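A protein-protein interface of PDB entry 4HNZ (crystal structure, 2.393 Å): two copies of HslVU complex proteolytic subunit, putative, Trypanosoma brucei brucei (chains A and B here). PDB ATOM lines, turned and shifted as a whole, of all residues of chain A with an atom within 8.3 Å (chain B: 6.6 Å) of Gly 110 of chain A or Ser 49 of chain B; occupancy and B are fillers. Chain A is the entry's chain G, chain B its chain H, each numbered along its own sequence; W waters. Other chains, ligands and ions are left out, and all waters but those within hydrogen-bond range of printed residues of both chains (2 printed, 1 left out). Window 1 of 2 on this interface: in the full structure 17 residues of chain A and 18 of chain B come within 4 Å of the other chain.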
ATOM      1  N   ALA A  75      -6.701   8.356 -24.179  1.00  0.00           N
ATOM      2  CA  ALA A  75      -6.083   7.479 -23.244  1.00  0.00           C
ATOM      3  C   ALA A  75      -5.404   6.344 -23.962  1.00  0.00           C
ATOM      4  O   ALA A  75      -4.252   6.008 -23.658  1.00  0.00           O
ATOM      5  CB  ALA A  75      -7.101   6.957 -22.235  1.00  0.00           C
ATOM      6  N   VAL A  76      -6.120   5.712 -24.865  1.00  0.00           N
ATOM      7  CA  VAL A  76      -5.539   4.603 -25.584  1.00  0.00           C
ATOM      8  C   VAL A  76      -4.346   5.014 -26.424  1.00  0.00           C
ATOM      9  O   VAL A  76      -3.327   4.318 -26.451  1.00  0.00           O
ATOM     10  CB  VAL A  76      -6.579   3.918 -26.467  1.00  0.00           C
ATOM     11  CG1 VAL A  76      -5.912   2.887 -27.395  1.00  0.00           C
ATOM     12  CG2 VAL A  76      -7.588   3.199 -25.575  1.00  0.00           C
ATOM     13  N   LEU A  78      -2.414   7.455 -25.749  1.00  0.00           N
ATOM     14  CA  LEU A  78      -1.335   7.705 -24.759  1.00  0.00           C
ATOM     15  C   LEU A  78      -0.667   6.422 -24.377  1.00  0.00           C
ATOM     16  O   LEU A  78       0.536   6.318 -24.398  1.00  0.00           O
ATOM     17  CB  LEU A  78      -1.891   8.371 -23.496  1.00  0.00           C
ATOM     18  CG  LEU A  78      -0.801   8.419 -22.433  1.00  0.00           C
ATOM     19  CD1 LEU A  78       0.182   9.542 -22.716  1.00  0.00           C
ATOM     20  CD2 LEU A  78      -1.368   8.552 -21.042  1.00  0.00           C
ATOM     21  N   ALA A  79      -1.464   5.423 -24.059  1.00  0.00           N
ATOM     22  CA  ALA A  79      -0.936   4.146 -23.590  1.00  0.00           C
ATOM     23  C   ALA A  79      -0.099   3.537 -24.684  1.00  0.00           C
ATOM     24  O   ALA A  79       1.010   3.019 -24.411  1.00  0.00           O
ATOM     25  CB  ALA A  79      -2.024   3.207 -23.171  1.00  0.00           C
ATOM     26  N   LYS A  80      -0.543   3.637 -25.930  1.00  0.00           N
ATOM     27  CA  LYS A  80       0.299   3.119 -27.078  1.00  0.00           C
ATOM     28  C   LYS A  80       1.643   3.788 -27.192  1.00  0.00           C
ATOM     29  O   LYS A  80       2.649   3.144 -27.414  1.00  0.00           O
ATOM     30  CB  LYS A  80      -0.420   3.288 -28.410  1.00  0.00           C
ATOM     31  CG  LYS A  80      -1.480   2.249 -28.622  1.00  0.00           C
ATOM     32  CD  LYS A  80      -2.517   2.660 -29.650  1.00  0.00           C
ATOM     33  CE  LYS A  80      -1.904   2.924 -31.002  1.00  0.00           C
ATOM     34  NZ  LYS A  80      -2.929   3.604 -31.840  1.00  0.00           N
ATOM     35  N   TRP A  82       3.171   5.465 -24.773  1.00  0.00           N
ATOM     36  CA  TRP A  82       3.871   5.150 -23.567  1.00  0.00           C
ATOM     37  C   TRP A  82       4.610   3.801 -23.723  1.00  0.00           C
ATOM     38  O   TRP A  82       5.767   3.678 -23.341  1.00  0.00           O
ATOM     39  CB  TRP A  82       2.862   5.081 -22.434  1.00  0.00           C
ATOM     40  CG  TRP A  82       3.389   4.932 -21.048  1.00  0.00           C
ATOM     41  CD1 TRP A  82       4.672   4.719 -20.662  1.00  0.00           C
ATOM     42  CD2 TRP A  82       2.622   4.980 -19.853  1.00  0.00           C
ATOM     43  NE1 TRP A  82       4.752   4.674 -19.316  1.00  0.00           N
ATOM     44  CE2 TRP A  82       3.513   4.816 -18.779  1.00  0.00           C
ATOM     45  CE3 TRP A  82       1.272   5.197 -19.583  1.00  0.00           C
ATOM     46  CZ2 TRP A  82       3.113   4.856 -17.448  1.00  0.00           C
ATOM     47  CZ3 TRP A  82       0.855   5.186 -18.286  1.00  0.00           C
ATOM     48  CH2 TRP A  82       1.772   5.001 -17.222  1.00  0.00           C
ATOM     49  N   ARG A  83       3.950   2.795 -24.252  1.00  0.00           N
ATOM     50  CA  ARG A  83       4.564   1.497 -24.326  1.00  0.00           C
ATOM     51  C   ARG A  83       5.623   1.384 -25.425  1.00  0.00           C
ATOM     52  O   ARG A  83       6.466   0.516 -25.336  1.00  0.00           O
ATOM     53  CB  ARG A  83       3.519   0.420 -24.550  1.00  0.00           C
ATOM     54  CG  ARG A  83       2.608   0.275 -23.356  1.00  0.00           C
ATOM     55  CD  ARG A  83       3.312  -0.358 -22.197  1.00  0.00           C
ATOM     56  NE  ARG A  83       3.715  -1.710 -22.572  1.00  0.00           N
ATOM     57  CZ  ARG A  83       4.467  -2.512 -21.832  1.00  0.00           C
ATOM     58  NH1 ARG A  83       4.905  -2.133 -20.653  1.00  0.00           N
ATOM     59  NH2 ARG A  83       4.731  -3.737 -22.267  1.00  0.00           N
ATOM     60  N   ARG A  89       8.958   4.660 -21.537  1.00  0.00           N
ATOM     61  CA  ARG A  89       8.990   3.401 -20.859  1.00  0.00           C
ATOM     62  C   ARG A  89       9.928   3.335 -19.662  1.00  0.00           C
ATOM     63  O   ARG A  89       9.856   2.403 -18.908  1.00  0.00           O
ATOM     64  CB  ARG A  89       9.368   2.299 -21.809  1.00  0.00           C
ATOM     65  CG  ARG A  89       8.136   1.686 -22.393  1.00  0.00           C
ATOM     66  CD  ARG A  89       8.536   0.431 -23.088  1.00  0.00           C
ATOM     67  NE  ARG A  89       8.607  -0.681 -22.144  1.00  0.00           N
ATOM     68  CZ  ARG A  89       7.954  -1.826 -22.282  1.00  0.00           C
ATOM     69  NH1 ARG A  89       7.134  -2.008 -23.323  1.00  0.00           N
ATOM     70  NH2 ARG A  89       8.133  -2.786 -21.379  1.00  0.00           N
ATOM     71  N   ALA A  93       4.591   4.998 -13.368  1.00  0.00           N
ATOM     72  CA  ALA A  93       3.455   5.757 -12.914  1.00  0.00           C
ATOM     73  C   ALA A  93       2.200   5.022 -13.275  1.00  0.00           C
ATOM     74  O   ALA A  93       2.183   4.216 -14.178  1.00  0.00           O
ATOM     75  CB  ALA A  93       3.456   7.127 -13.580  1.00  0.00           C
ATOM     76  N   GLU A 105      -8.298   4.262 -16.232  1.00  0.00           N
ATOM     77  CA  GLU A 105      -7.085   4.003 -15.543  1.00  0.00           C
ATOM     78  C   GLU A 105      -6.084   3.559 -16.589  1.00  0.00           C
ATOM     79  O   GLU A 105      -6.398   2.704 -17.457  1.00  0.00           O
ATOM     80  CB  GLU A 105      -7.350   2.947 -14.469  1.00  0.00           C
ATOM     81  CG  GLU A 105      -6.141   2.165 -14.003  1.00  0.00           C
ATOM     82  CD  GLU A 105      -6.488   1.018 -13.057  1.00  0.00           C
ATOM     83  OE1 GLU A 105      -7.648   0.894 -12.634  1.00  0.00           O
ATOM     84  OE2 GLU A 105      -5.566   0.204 -12.755  1.00  0.00           O
ATOM     85  N   ILE A 106      -4.888   4.103 -16.502  1.00  0.00           N
ATOM     86  CA  ILE A 106      -3.817   3.750 -17.428  1.00  0.00           C
ATOM     87  C   ILE A 106      -2.545   3.476 -16.708  1.00  0.00           C
ATOM     88  O   ILE A 106      -2.164   4.217 -15.821  1.00  0.00           O
ATOM     89  CB  ILE A 106      -3.497   4.929 -18.381  1.00  0.00           C
ATOM     90  CG1 ILE A 106      -4.773   5.465 -19.000  1.00  0.00           C
ATOM     91  CG2 ILE A 106      -2.552   4.472 -19.476  1.00  0.00           C
ATOM     92  CD1 ILE A 106      -4.624   6.877 -19.524  1.00  0.00           C
ATOM     93  N   ASP A 107      -1.931   2.357 -16.987  1.00  0.00           N
ATOM     94  CA  ASP A 107      -0.692   1.982 -16.251  1.00  0.00           C
ATOM     95  C   ASP A 107       0.449   1.719 -17.212  1.00  0.00           C
ATOM     96  O   ASP A 107       0.259   1.681 -18.450  1.00  0.00           O
ATOM     97  CB  ASP A 107      -0.949   0.837 -15.273  1.00  0.00           C
ATOM     98  CG  ASP A 107      -1.288  -0.462 -15.939  1.00  0.00           C
ATOM     99  OD1 ASP A 107      -0.834  -0.764 -17.098  1.00  0.00           O
ATOM    100  OD2 ASP A 107      -1.930  -1.275 -15.250  1.00  0.00           O
ATOM    101  N   GLY A 108       1.638   1.520 -16.634  1.00  0.00           N
ATOM    102  CA  GLY A 108       2.849   1.278 -17.401  1.00  0.00           C
ATOM    103  C   GLY A 108       2.912  -0.050 -18.139  1.00  0.00           C
ATOM    104  O   GLY A 108       3.766  -0.232 -18.988  1.00  0.00           O
ATOM    105  N   GLN A 109       2.057  -0.994 -17.779  1.00  0.00           N
ATOM    106  CA  GLN A 109       1.952  -2.266 -18.522  1.00  0.00           C
ATOM    107  C   GLN A 109       1.118  -2.096 -19.765  1.00  0.00           C
ATOM    108  O   GLN A 109       1.049  -2.999 -20.594  1.00  0.00           O
ATOM    109  CB  GLN A 109       1.368  -3.362 -17.646  1.00  0.00           C
ATOM    110  CG  GLN A 109       2.430  -4.096 -16.852  1.00  0.00           C
ATOM    111  CD  GLN A 109       3.220  -3.161 -15.975  1.00  0.00           C
ATOM    112  OE1 GLN A 109       4.430  -3.015 -16.134  1.00  0.00           O
ATOM    113  NE2 GLN A 109       2.537  -2.498 -15.058  1.00  0.00           N
ATOM    114  N   GLY A 110       0.460  -0.948 -19.912  1.00  0.00           N
ATOM    115  CA  GLY A 110      -0.341  -0.701 -21.107  1.00  0.00           C
ATOM    116  C   GLY A 110      -1.787  -1.089 -20.992  1.00  0.00           C
ATOM    117  O   GLY A 110      -2.505  -1.107 -21.988  1.00  0.00           O
ATOM    118  N   ASN A 111      -2.240  -1.350 -19.766  1.00  0.00           N
ATOM    119  CA  ASN A 111      -3.668  -1.537 -19.543  1.00  0.00           C
ATOM    120  C   ASN A 111      -4.387  -0.208 -19.553  1.00  0.00           C
ATOM    121  O   ASN A 111      -3.901   0.787 -19.068  1.00  0.00           O
ATOM    122  CB  ASN A 111      -3.942  -2.238 -18.205  1.00  0.00           C
ATOM    123  CG  ASN A 111      -3.240  -3.605 -18.084  1.00  0.00           C
ATOM    124  OD1 ASN A 111      -3.529  -4.534 -18.848  1.00  0.00           O
ATOM    125  ND2 ASN A 111      -2.315  -3.723 -17.104  1.00  0.00           N
ATOM    126  N   VAL A 112      -5.578  -0.216 -20.104  1.00  0.00           N
ATOM    127  CA  VAL A 112      -6.475   0.894 -20.060  1.00  0.00           C
ATOM    128  C   VAL A 112      -7.771   0.288 -19.493  1.00  0.00           C
ATOM    129  O   VAL A 112      -8.384  -0.486 -20.148  1.00  0.00           O
ATOM    130  CB  VAL A 112      -6.709   1.461 -21.454  1.00  0.00           C
ATOM    131  CG1 VAL A 112      -7.695   2.607 -21.405  1.00  0.00           C
ATOM    132  CG2 VAL A 112      -5.402   1.948 -22.034  1.00  0.00           C
ATOM    133  N   ILE A 113      -8.145   0.666 -18.281  1.00  0.00           N
ATOM    134  CA  ILE A 113      -9.186  -0.009 -17.545  1.00  0.00           C
ATOM    135  C   ILE A 113     -10.247   1.008 -17.262  1.00  0.00           C
ATOM    136  O   ILE A 113      -9.952   2.086 -16.779  1.00  0.00           O
ATOM    137  CB  ILE A 113      -8.634  -0.563 -16.250  1.00  0.00           C
ATOM    138  CG1 ILE A 113      -7.817  -1.822 -16.566  1.00  0.00           C
ATOM    139  CG2 ILE A 113      -9.725  -0.840 -15.223  1.00  0.00           C
ATOM    140  CD1 ILE A 113      -6.653  -2.002 -15.627  1.00  0.00           C
ATOM    141  N   PHE B  46      -6.622 -11.536 -28.504  1.00  0.00           N
ATOM    142  CA  PHE B  46      -5.315 -11.194 -27.891  1.00  0.00           C
ATOM    143  C   PHE B  46      -5.197 -11.539 -26.429  1.00  0.00           C
ATOM    144  O   PHE B  46      -6.134 -11.424 -25.659  1.00  0.00           O
ATOM    145  CB  PHE B  46      -4.926  -9.698 -28.155  1.00  0.00           C
ATOM    146  CG  PHE B  46      -5.770  -8.670 -27.412  1.00  0.00           C
ATOM    147  CD1 PHE B  46      -5.431  -8.238 -26.117  1.00  0.00           C
ATOM    148  CD2 PHE B  46      -6.879  -8.060 -28.042  1.00  0.00           C
ATOM    149  CE1 PHE B  46      -6.203  -7.259 -25.434  1.00  0.00           C
ATOM    150  CE2 PHE B  46      -7.640  -7.083 -27.366  1.00  0.00           C
ATOM    151  CZ  PHE B  46      -7.308  -6.688 -26.060  1.00  0.00           C
ATOM    152  N   ALA B  47      -4.033 -12.036 -26.074  1.00  0.00           N
ATOM    153  CA  ALA B  47      -3.555 -11.999 -24.701  1.00  0.00           C
ATOM    154  C   ALA B  47      -2.511 -10.896 -24.603  1.00  0.00           C
ATOM    155  O   ALA B  47      -1.689 -10.735 -25.523  1.00  0.00           O
ATOM    156  CB  ALA B  47      -2.940 -13.334 -24.325  1.00  0.00           C
ATOM    157  N   GLY B  48      -2.533 -10.142 -23.502  1.00  0.00           N
ATOM    158  CA  GLY B  48      -1.671  -9.001 -23.288  1.00  0.00           C
ATOM    159  C   GLY B  48      -2.486  -7.745 -23.032  1.00  0.00           C
ATOM    160  O   GLY B  48      -3.708  -7.778 -23.031  1.00  0.00           O
ATOM    161  N   SER B  49      -1.801  -6.649 -22.752  1.00  0.00           N
ATOM    162  CA  SER B  49      -2.459  -5.433 -22.359  1.00  0.00           C
ATOM    163  C   SER B  49      -3.088  -4.778 -23.569  1.00  0.00           C
ATOM    164  O   SER B  49      -2.676  -5.008 -24.715  1.00  0.00           O
ATOM    165  CB  SER B  49      -1.440  -4.455 -21.743  1.00  0.00           C
ATOM    166  OG  SER B  49      -0.549  -3.980 -22.750  1.00  0.00           O
ATOM    167  N   THR B  50      -4.084  -3.980 -23.298  1.00  0.00           N
ATOM    168  CA  THR B  50      -4.781  -3.265 -24.323  1.00  0.00           C
ATOM    169  C   THR B  50      -3.808  -2.577 -25.265  1.00  0.00           C
ATOM    170  O   THR B  50      -3.910  -2.736 -26.491  1.00  0.00           O
ATOM    171  CB  THR B  50      -5.625  -2.180 -23.662  1.00  0.00           C
ATOM    172  OG1 THR B  50      -6.514  -2.811 -22.721  1.00  0.00           O
ATOM    173  CG2 THR B  50      -6.456  -1.382 -24.714  1.00  0.00           C
ATOM    174  N   ALA B  51      -2.909  -1.753 -24.715  1.00  0.00           N
ATOM    175  CA  ALA B  51      -2.041  -0.989 -25.559  1.00  0.00           C
ATOM    176  C   ALA B  51      -1.099  -1.880 -26.379  1.00  0.00           C
ATOM    177  O   ALA B  51      -0.803  -1.576 -27.542  1.00  0.00           O
ATOM    178  CB  ALA B  51      -1.251   0.026 -24.740  1.00  0.00           C
ATOM    179  N   ASP B  52      -0.581  -2.939 -25.754  1.00  0.00           N
ATOM    180  CA  ASP B  52       0.385  -3.783 -26.436  1.00  0.00           C
ATOM    181  C   ASP B  52      -0.289  -4.469 -27.564  1.00  0.00           C
ATOM    182  O   ASP B  52       0.213  -4.454 -28.680  1.00  0.00           O
ATOM    183  CB  ASP B  52       0.982  -4.804 -25.513  1.00  0.00           C
ATOM    184  CG  ASP B  52       2.042  -4.211 -24.581  1.00  0.00           C
ATOM    185  OD1 ASP B  52       1.925  -3.026 -24.176  1.00  0.00           O
ATOM    186  OD2 ASP B  52       2.916  -4.982 -24.138  1.00  0.00           O
ATOM    187  N   ALA B  53      -1.453  -5.043 -27.292  1.00  0.00           N
ATOM    188  CA  ALA B  53      -2.189  -5.788 -28.283  1.00  0.00           C
ATOM    189  C   ALA B  53      -2.709  -4.931 -29.440  1.00  0.00           C
ATOM    190  O   ALA B  53      -2.572  -5.311 -30.602  1.00  0.00           O
ATOM    191  CB  ALA B  53      -3.352  -6.480 -27.651  1.00  0.00           C
ATOM    192  N   ILE B  54      -3.202  -3.736 -29.142  1.00  0.00           N
ATOM    193  CA  ILE B  54      -3.658  -2.805 -30.184  1.00  0.00           C
ATOM    194  C   ILE B  54      -2.534  -2.290 -31.082  1.00  0.00           C
ATOM    195  O   ILE B  54      -2.705  -2.181 -32.272  1.00  0.00           O
ATOM    196  CB  ILE B  54      -4.436  -1.663 -29.530  1.00  0.00           C
ATOM    197  CG1 ILE B  54      -5.780  -2.235 -29.041  1.00  0.00           C
ATOM    198  CG2 ILE B  54      -4.659  -0.544 -30.509  1.00  0.00           C
ATOM    199  CD1 ILE B  54      -6.681  -1.214 -28.374  1.00  0.00           C
ATOM    200  N   GLU B  92       4.468  -7.163 -24.950  1.00  0.00           N
ATOM    201  CA  GLU B  92       4.182  -8.521 -24.601  1.00  0.00           C
ATOM    202  C   GLU B  92       2.744  -8.822 -24.994  1.00  0.00           C
ATOM    203  O   GLU B  92       1.802  -8.250 -24.420  1.00  0.00           O
ATOM    204  CB  GLU B  92       4.339  -8.709 -23.122  1.00  0.00           C
ATOM    205  CG  GLU B  92       5.785  -8.704 -22.667  1.00  0.00           C
ATOM    206  CD  GLU B  92       5.864  -8.876 -21.146  1.00  0.00           C
ATOM    207  OE1 GLU B  92       6.283  -7.914 -20.470  1.00  0.00           O
ATOM    208  OE2 GLU B  92       5.457  -9.968 -20.647  1.00  0.00           O
ATOM    209  N   ALA B  93       2.572  -9.770 -25.916  1.00  0.00           N
ATOM    210  CA  ALA B  93       1.258 -10.161 -26.346  1.00  0.00           C
ATOM    211  C   ALA B  93       1.311 -11.444 -27.126  1.00  0.00           C
ATOM    212  O   ALA B  93       2.325 -11.800 -27.595  1.00  0.00           O
ATOM    213  CB  ALA B  93       0.688  -9.055 -27.212  1.00  0.00           C
HETATM  214  O   HOH W   1      -7.488  -3.080 -20.096  1.00  0.00           O
HETATM  215  O   HOH W   2       2.601  -4.814 -20.937  1.00  0.00           O
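The side-chain hydroxyl (OG) of Ser 49 of chain B sits at hydrogen-bond distance from the backbone carbonyl oxygen (O) of Gln 109 of chain A. O of Gly 110 of chain A sits at hydrogen-bond distance from N of Ala 51 of chain B, at 2.8 Å. The guanidinium group (NE) of Arg 83 of chain A lies within salt-bridge range of the side-chain carboxylate (OD1) of Asp 52 of chain B (2.7 Å).
Among the printed residues, pairs that only touch across the chains: Gly 110 of chain A with Ser 49 of chain B (3.5 Å), Gly 110 of chain A with Thr 50 of chain B (3.5 Å), Asn 111 of chain A with Ser 49 of chain B (3.6 Å), Ala 79 of chain A with Ala 51 of chain B (3.6 Å), Gln 109 of chain A with Asp 52 of chain B (3.7 Å), Val 112 of chain A with Thr 50 of chain B (3.8 Å), Lys 80 of chain A with Ala 51 of chain B (3.9 Å) and Lys 80 of chain A with Ile 54 of chain B (3.9 Å).
The side-chain carboxylate of Asp 107 of chain A sits at hydrogen-bond distance from the backbone NH of Asn 111 of chain A (3.1 Å). OD1 of Asp 107 of chain A is in hydrogen-bond range of N of Gln 109 of chain A (3.0 Å). OD2 of Asp 52 of chain B is in hydrogen-bond range of N of Glu 92 of chain B (2.8 Å). The side-chain hydroxyl (OG) of Ser 49 of chain B is in hydrogen-bond range of the side-chain carboxylate (OD1) of Asp 52 of chain B. O of Arg 83 of chain A lies close to NH1 of Arg 89 of chain A (3.3 Å). O of Gly 108 of chain A sits at hydrogen-bond distance from NH1 of Arg 83 of chain A, 2.8 Å away.
Water W2 lies within hydrogen-bond range of O of Gln 109 of chain A (2.4 Å), NH2 of Arg 83 of chain A (2.7 Å) and OD2 of Asp 52 of chain B (3.2 Å). Water W1 lies within hydrogen-bond range of O of Val 112 of chain A and OG1 of Thr 50 of chain B.
Of the printed residues of chain B, Lys 80 of chain A touches Ala 51 and Ile 54. Trp 82 of chain A touches none of the printed residues of chain B. Of chain B, only Ser 49 (3.5 Å), Thr 50 (3.5 Å) and Ala 51 (2.8 Å) come within 4 Å of Gly 110 of chain A. Printed residues of chain B within 4 Å of Asn 111 of chain A: Ser 49. Of the printed residues of chain A, Thr 50 of chain B touches Gly 110 and Val 112. The nearest residue of chain B that does not touch Gly 110 of chain A is Asp 52 of chain B (4.5 Å). The nearest printed residue of chain B that does not touch Arg 83 of chain A is Ala 51 of chain B (4.1 Å).
1 position is printed for both chains.
Of the 11 printed residues of chain B, 5 touch a printed residue of chain A. Hydrophobic or aromatic side chains of chain B within 4 Å of the printed part of chain A: Ala 51 and Ile 54. Of the 18 printed residues of chain A, 7 touch a printed residue of chain B. Hydrophobic or aromatic side chains of chain A that line the printed part of chain B: Ala 79.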
